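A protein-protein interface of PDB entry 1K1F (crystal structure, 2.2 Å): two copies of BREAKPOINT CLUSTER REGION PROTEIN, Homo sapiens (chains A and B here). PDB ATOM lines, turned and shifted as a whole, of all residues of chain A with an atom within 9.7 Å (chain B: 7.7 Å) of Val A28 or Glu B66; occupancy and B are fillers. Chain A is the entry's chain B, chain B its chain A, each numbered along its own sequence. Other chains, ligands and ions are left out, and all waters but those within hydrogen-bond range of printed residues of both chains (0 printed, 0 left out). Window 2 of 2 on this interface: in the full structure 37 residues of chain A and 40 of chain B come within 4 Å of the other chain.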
ATOM      1  N   VAL A   2     -10.472  -6.828 -13.605  1.00  0.00           N
ATOM      2  CA  VAL A   2      -9.891  -6.070 -12.500  1.00  0.00           C
ATOM      3  C   VAL A   2      -9.183  -4.884 -13.153  1.00  0.00           C
ATOM      4  O   VAL A   2      -8.141  -4.430 -12.687  1.00  0.00           O
ATOM      5  CB  VAL A   2      -8.851  -6.920 -11.726  1.00  0.00           C
ATOM      6  CG1 VAL A   2      -8.520  -6.275 -10.396  1.00  0.00           C
ATOM      7  CG2 VAL A   2      -9.383  -8.321 -11.507  1.00  0.00           C
ATOM      8  N   GLU A  24       2.277  -5.136  -9.989  1.00  0.00           N
ATOM      9  CA  GLU A  24       1.990  -6.522 -10.304  1.00  0.00           C
ATOM     10  C   GLU A  24       0.683  -6.985  -9.665  1.00  0.00           C
ATOM     11  O   GLU A  24       0.630  -8.008  -8.972  1.00  0.00           O
ATOM     12  CB  GLU A  24       3.169  -7.416  -9.874  1.00  0.00           C
ATOM     13  CG  GLU A  24       2.974  -8.904 -10.152  1.00  0.00           C
ATOM     14  CD  GLU A  24       2.246  -9.150 -11.464  1.00  0.00           C
ATOM     15  OE1 GLU A  24       2.727  -8.640 -12.498  1.00  0.00           O
ATOM     16  OE2 GLU A  24       1.200  -9.841 -11.461  1.00  0.00           O
ATOM     17  N   LEU A  25      -0.378  -6.226  -9.914  1.00  0.00           N
ATOM     18  CA  LEU A  25      -1.682  -6.556  -9.379  1.00  0.00           C
ATOM     19  C   LEU A  25      -2.283  -7.731 -10.126  1.00  0.00           C
ATOM     20  O   LEU A  25      -2.593  -7.653 -11.324  1.00  0.00           O
ATOM     21  CB  LEU A  25      -2.646  -5.372  -9.476  1.00  0.00           C
ATOM     22  CG  LEU A  25      -2.226  -4.055  -8.833  1.00  0.00           C
ATOM     23  CD1 LEU A  25      -3.413  -3.103  -8.835  1.00  0.00           C
ATOM     24  CD2 LEU A  25      -1.745  -4.285  -7.420  1.00  0.00           C
ATOM     25  N   ARG A  26      -2.417  -8.830  -9.405  1.00  0.00           N
ATOM     26  CA  ARG A  26      -3.031 -10.037  -9.921  1.00  0.00           C
ATOM     27  C   ARG A  26      -3.724 -10.543  -8.681  1.00  0.00           C
ATOM     28  O   ARG A  26      -4.957 -10.570  -8.566  1.00  0.00           O
ATOM     29  CB  ARG A  26      -1.989 -11.089 -10.384  1.00  0.00           C
ATOM     30  CG  ARG A  26      -0.878 -11.467  -9.366  1.00  0.00           C
ATOM     31  CD  ARG A  26      -0.578 -12.983  -9.316  1.00  0.00           C
ATOM     32  NE  ARG A  26       0.860 -13.272  -9.367  1.00  0.00           N
ATOM     33  CZ  ARG A  26       1.477 -14.214  -8.652  1.00  0.00           C
ATOM     34  NH1 ARG A  26       0.793 -14.975  -7.808  1.00  0.00           N
ATOM     35  NH2 ARG A  26       2.783 -14.409  -8.795  1.00  0.00           N
ATOM     36  N   SER A  27      -2.864 -10.858  -7.729  1.00  0.00           N
ATOM     37  CA  SER A  27      -3.213 -11.432  -6.459  1.00  0.00           C
ATOM     38  C   SER A  27      -3.565 -10.460  -5.338  1.00  0.00           C
ATOM     39  O   SER A  27      -3.324  -9.254  -5.412  1.00  0.00           O
ATOM     40  CB  SER A  27      -2.049 -12.337  -6.030  1.00  0.00           C
ATOM     41  OG  SER A  27      -1.690 -12.160  -4.675  1.00  0.00           O
ATOM     42  N   VAL A  28      -4.181 -11.014  -4.306  1.00  0.00           N
ATOM     43  CA  VAL A  28      -4.523 -10.263  -3.125  1.00  0.00           C
ATOM     44  C   VAL A  28      -3.132 -10.016  -2.530  1.00  0.00           C
ATOM     45  O   VAL A  28      -2.832  -8.942  -2.012  1.00  0.00           O
ATOM     46  CB  VAL A  28      -5.403 -11.137  -2.185  1.00  0.00           C
ATOM     47  CG1 VAL A  28      -5.333 -10.639  -0.747  1.00  0.00           C
ATOM     48  CG2 VAL A  28      -6.859 -11.137  -2.694  1.00  0.00           C
ATOM     49  N   GLY A  29      -2.271 -11.027  -2.661  1.00  0.00           N
ATOM     50  CA  GLY A  29      -0.911 -10.952  -2.144  1.00  0.00           C
ATOM     51  C   GLY A  29      -0.107  -9.825  -2.751  1.00  0.00           C
ATOM     52  O   GLY A  29       0.708  -9.207  -2.072  1.00  0.00           O
ATOM     53  N   ASP A  30      -0.331  -9.552  -4.031  1.00  0.00           N
ATOM     54  CA  ASP A  30       0.396  -8.477  -4.718  1.00  0.00           C
ATOM     55  C   ASP A  30      -0.157  -7.104  -4.343  1.00  0.00           C
ATOM     56  O   ASP A  30       0.599  -6.149  -4.173  1.00  0.00           O
ATOM     57  CB  ASP A  30       0.320  -8.678  -6.229  1.00  0.00           C
ATOM     58  CG  ASP A  30       1.152  -9.870  -6.699  1.00  0.00           C
ATOM     59  OD1 ASP A  30       2.368  -9.713  -6.937  1.00  0.00           O
ATOM     60  OD2 ASP A  30       0.593 -10.981  -6.821  1.00  0.00           O
ATOM     61  N   ILE A  31      -1.475  -7.006  -4.227  1.00  0.00           N
ATOM     62  CA  ILE A  31      -2.087  -5.758  -3.819  1.00  0.00           C
ATOM     63  C   ILE A  31      -1.496  -5.371  -2.454  1.00  0.00           C
ATOM     64  O   ILE A  31      -0.951  -4.287  -2.317  1.00  0.00           O
ATOM     65  CB  ILE A  31      -3.601  -5.908  -3.715  1.00  0.00           C
ATOM     66  CG1 ILE A  31      -4.183  -6.104  -5.125  1.00  0.00           C
ATOM     67  CG2 ILE A  31      -4.205  -4.676  -3.091  1.00  0.00           C
ATOM     68  CD1 ILE A  31      -5.662  -6.542  -5.138  1.00  0.00           C
ATOM     69  N   GLU A  32      -1.586  -6.263  -1.463  1.00  0.00           N
ATOM     70  CA  GLU A  32      -1.027  -6.006  -0.129  1.00  0.00           C
ATOM     71  C   GLU A  32       0.419  -5.521  -0.222  1.00  0.00           C
ATOM     72  O   GLU A  32       0.761  -4.461   0.311  1.00  0.00           O
ATOM     73  CB  GLU A  32      -1.064  -7.272   0.735  1.00  0.00           C
ATOM     74  CG  GLU A  32      -2.476  -7.804   1.048  1.00  0.00           C
ATOM     75  CD  GLU A  32      -2.453  -9.017   1.971  1.00  0.00           C
ATOM     76  OE1 GLU A  32      -1.389  -9.665   2.082  1.00  0.00           O
ATOM     77  OE2 GLU A  32      -3.502  -9.341   2.579  1.00  0.00           O
ATOM     78  N   GLN A  33       1.264  -6.298  -0.902  1.00  0.00           N
ATOM     79  CA  GLN A  33       2.674  -5.960  -1.066  1.00  0.00           C
ATOM     80  C   GLN A  33       2.847  -4.544  -1.589  1.00  0.00           C
ATOM     81  O   GLN A  33       3.628  -3.762  -1.049  1.00  0.00           O
ATOM     82  CB  GLN A  33       3.364  -6.954  -2.021  1.00  0.00           C
ATOM     83  CG  GLN A  33       4.776  -6.531  -2.428  1.00  0.00           C
ATOM     84  CD  GLN A  33       5.793  -7.638  -2.265  1.00  0.00           C
ATOM     85  OE1 GLN A  33       5.578  -8.762  -2.732  1.00  0.00           O
ATOM     86  NE2 GLN A  33       6.919  -7.331  -1.603  1.00  0.00           N
ATOM     87  N   GLU A  34       2.108  -4.210  -2.635  1.00  0.00           N
ATOM     88  CA  GLU A  34       2.191  -2.882  -3.205  1.00  0.00           C
ATOM     89  C   GLU A  34       1.644  -1.798  -2.265  1.00  0.00           C
ATOM     90  O   GLU A  34       2.177  -0.683  -2.209  1.00  0.00           O
ATOM     91  CB  GLU A  34       1.437  -2.849  -4.523  1.00  0.00           C
ATOM     92  CG  GLU A  34       1.616  -1.564  -5.295  1.00  0.00           C
ATOM     93  CD  GLU A  34       3.067  -1.316  -5.690  1.00  0.00           C
ATOM     94  OE1 GLU A  34       3.636  -2.183  -6.392  1.00  0.00           O
ATOM     95  OE2 GLU A  34       3.633  -0.262  -5.302  1.00  0.00           O
ATOM     96  N   LEU A  35       0.577  -2.115  -1.535  1.00  0.00           N
ATOM     97  CA  LEU A  35      -0.022  -1.152  -0.624  1.00  0.00           C
ATOM     98  C   LEU A  35       1.007  -0.841   0.450  1.00  0.00           C
ATOM     99  O   LEU A  35       1.090   0.271   0.971  1.00  0.00           O
ATOM    100  CB  LEU A  35      -1.275  -1.755   0.012  1.00  0.00           C
ATOM    101  CG  LEU A  35      -2.010  -0.879   1.029  1.00  0.00           C
ATOM    102  CD1 LEU A  35      -2.577   0.298   0.295  1.00  0.00           C
ATOM    103  CD2 LEU A  35      -3.154  -1.634   1.687  1.00  0.00           C
ATOM    104  N   GLU A  36       1.817  -1.849   0.740  1.00  0.00           N
ATOM    105  CA  GLU A  36       2.840  -1.757   1.755  1.00  0.00           C
ATOM    106  C   GLU A  36       4.050  -0.922   1.293  1.00  0.00           C
ATOM    107  O   GLU A  36       4.597  -0.145   2.074  1.00  0.00           O
ATOM    108  CB  GLU A  36       3.222  -3.188   2.158  1.00  0.00           C
ATOM    109  CG  GLU A  36       3.486  -3.415   3.634  1.00  0.00           C
ATOM    110  CD  GLU A  36       2.521  -2.691   4.554  1.00  0.00           C
ATOM    111  OE1 GLU A  36       1.394  -3.181   4.779  1.00  0.00           O
ATOM    112  OE2 GLU A  36       2.900  -1.607   5.057  1.00  0.00           O
ATOM    113  N   GLN B  60      -6.003   0.248  -1.176  1.00  0.00           N
ATOM    114  CA  GLN B  60      -6.826  -0.294  -0.104  1.00  0.00           C
ATOM    115  C   GLN B  60      -8.266  -0.510  -0.568  1.00  0.00           C
ATOM    116  O   GLN B  60      -8.944  -1.419  -0.083  1.00  0.00           O
ATOM    117  CB  GLN B  60      -6.764   0.559   1.177  1.00  0.00           C
ATOM    118  CG  GLN B  60      -6.590   2.029   1.016  1.00  0.00           C
ATOM    119  CD  GLN B  60      -6.297   2.689   2.352  1.00  0.00           C
ATOM    120  OE1 GLN B  60      -5.365   2.294   3.052  1.00  0.00           O
ATOM    121  NE2 GLN B  60      -7.092   3.695   2.716  1.00  0.00           N
ATOM    122  N   THR B  61      -8.731   0.316  -1.509  1.00  0.00           N
ATOM    123  CA  THR B  61     -10.069   0.160  -2.079  1.00  0.00           C
ATOM    124  C   THR B  61     -10.120  -1.203  -2.783  1.00  0.00           C
ATOM    125  O   THR B  61     -11.129  -1.900  -2.733  1.00  0.00           O
ATOM    126  CB  THR B  61     -10.361   1.265  -3.133  1.00  0.00           C
ATOM    127  OG1 THR B  61     -10.384   2.543  -2.495  1.00  0.00           O
ATOM    128  CG2 THR B  61     -11.709   1.045  -3.799  1.00  0.00           C
ATOM    129  N   LEU B  62      -9.027  -1.596  -3.432  1.00  0.00           N
ATOM    130  CA  LEU B  62      -8.995  -2.891  -4.132  1.00  0.00           C
ATOM    131  C   LEU B  62      -9.055  -4.125  -3.242  1.00  0.00           C
ATOM    132  O   LEU B  62      -9.908  -4.986  -3.455  1.00  0.00           O
ATOM    133  CB  LEU B  62      -7.761  -3.015  -5.026  1.00  0.00           C
ATOM    134  CG  LEU B  62      -7.682  -2.133  -6.263  1.00  0.00           C
ATOM    135  CD1 LEU B  62      -6.379  -2.424  -6.993  1.00  0.00           C
ATOM    136  CD2 LEU B  62      -8.868  -2.422  -7.179  1.00  0.00           C
ATOM    137  N   LEU B  63      -8.157  -4.247  -2.261  1.00  0.00           N
ATOM    138  CA  LEU B  63      -8.207  -5.443  -1.419  1.00  0.00           C
ATOM    139  C   LEU B  63      -9.491  -5.512  -0.619  1.00  0.00           C
ATOM    140  O   LEU B  63      -9.861  -6.570  -0.127  1.00  0.00           O
ATOM    141  CB  LEU B  63      -7.009  -5.547  -0.467  1.00  0.00           C
ATOM    142  CG  LEU B  63      -6.789  -4.505   0.613  1.00  0.00           C
ATOM    143  CD1 LEU B  63      -5.837  -5.024   1.670  1.00  0.00           C
ATOM    144  CD2 LEU B  63      -6.212  -3.301  -0.035  1.00  0.00           C
ATOM    145  N   ALA B  64     -10.172  -4.382  -0.484  1.00  0.00           N
ATOM    146  CA  ALA B  64     -11.431  -4.365   0.236  1.00  0.00           C
ATOM    147  C   ALA B  64     -12.477  -5.098  -0.604  1.00  0.00           C
ATOM    148  O   ALA B  64     -13.219  -5.924  -0.074  1.00  0.00           O
ATOM    149  CB  ALA B  64     -11.868  -2.937   0.497  1.00  0.00           C
ATOM    150  N   LYS B  65     -12.526  -4.808  -1.908  1.00  0.00           N
ATOM    151  CA  LYS B  65     -13.494  -5.447  -2.805  1.00  0.00           C
ATOM    152  C   LYS B  65     -13.055  -6.852  -3.224  1.00  0.00           C
ATOM    153  O   LYS B  65     -13.571  -7.424  -4.194  1.00  0.00           O
ATOM    154  CB  LYS B  65     -13.742  -4.587  -4.059  1.00  0.00           C
ATOM    155  CG  LYS B  65     -12.660  -4.642  -5.127  1.00  0.00           C
ATOM    156  CD  LYS B  65     -13.027  -3.730  -6.297  1.00  0.00           C
ATOM    157  CE  LYS B  65     -12.005  -3.806  -7.426  1.00  0.00           C
ATOM    158  NZ  LYS B  65     -12.253  -2.765  -8.483  1.00  0.00           N
ATOM    159  N   GLU B  66     -12.101  -7.397  -2.480  1.00  0.00           N
ATOM    160  CA  GLU B  66     -11.581  -8.734  -2.729  1.00  0.00           C
ATOM    161  C   GLU B  66     -11.214  -9.351  -1.385  1.00  0.00           C
ATOM    162  O   GLU B  66     -10.685 -10.458  -1.313  1.00  0.00           O
ATOM    163  CB  GLU B  66     -10.348  -8.651  -3.631  1.00  0.00           C
ATOM    164  CG  GLU B  66      -9.718  -9.980  -4.012  1.00  0.00           C
ATOM    165  CD  GLU B  66      -8.570  -9.802  -5.001  1.00  0.00           C
ATOM    166  OE1 GLU B  66      -7.985  -8.697  -5.046  1.00  0.00           O
ATOM    167  OE2 GLU B  66      -8.249 -10.770  -5.720  1.00  0.00           O
ATOM    168  N   LYS B  67     -11.522  -8.617  -0.321  1.00  0.00           N
ATOM    169  CA  LYS B  67     -11.224  -9.036   1.037  1.00  0.00           C
ATOM    170  C   LYS B  67     -12.260 -10.061   1.495  1.00  0.00           C
ATOM    171  O   LYS B  67     -11.839 -11.161   1.919  1.00  0.00           O
ATOM    172  CB  LYS B  67     -11.245  -7.816   1.964  1.00  0.00           C
ATOM    173  CG  LYS B  67     -10.356  -7.914   3.196  1.00  0.00           C
ATOM    174  CD  LYS B  67      -8.879  -7.883   2.820  1.00  0.00           C
ATOM    175  CE  LYS B  67      -7.994  -7.846   4.063  1.00  0.00           C
ATOM    176  NZ  LYS B  67      -6.534  -7.858   3.754  1.00  0.00           N
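The side-chain carboxylate (OE2) of Glu A32 lies within salt-bridge range of the side-chain amino group (NZ) of Lys B67 (3.6 Å).
Among the printed residues, merely in contact across the chains: Leu A25 with Leu B62 (3.6 Å), Val A28 with Glu B66 (3.2 Å), Ile A31 with Leu B63 (3.9 Å), Ile A31 with Glu B66 (3.2 Å), Leu A35 with Gln B60 (3.7 Å) and Leu A35 with Leu B63 (3.9 Å).
Val A28 touches just one residue of chain B: Glu B66 (3.2 Å).
No residue of chain B comes within 4 Å of Gly A29.
Of the printed residues of chain B, Ile A31 touches Leu B63 (3.9 Å) and Glu B66 (3.2 Å).
Of the printed residues of chain A, Leu B63 touches Ile A31 and Leu A35.
Lys B65 touches none of the printed residues of chain A.
Glu B66 touches just these residues of chain A: Val A28 and Ile A31.
The nearest printed residue of chain A that does not touch Leu B62 is Ile A31 (4.1 Å).
Among the printed residues, 7 pairs touch across the chains.
Among the printed residues, Asp or Glu carboxylates within 4 Å of a Lys or Arg side-chain nitrogen of the other chain: Glu A32 with Lys B67.
No position is printed for both chains.
Of the 7 pairs that touch across the chains among the printed residues, none has its exchanged pair printed and touching as well.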
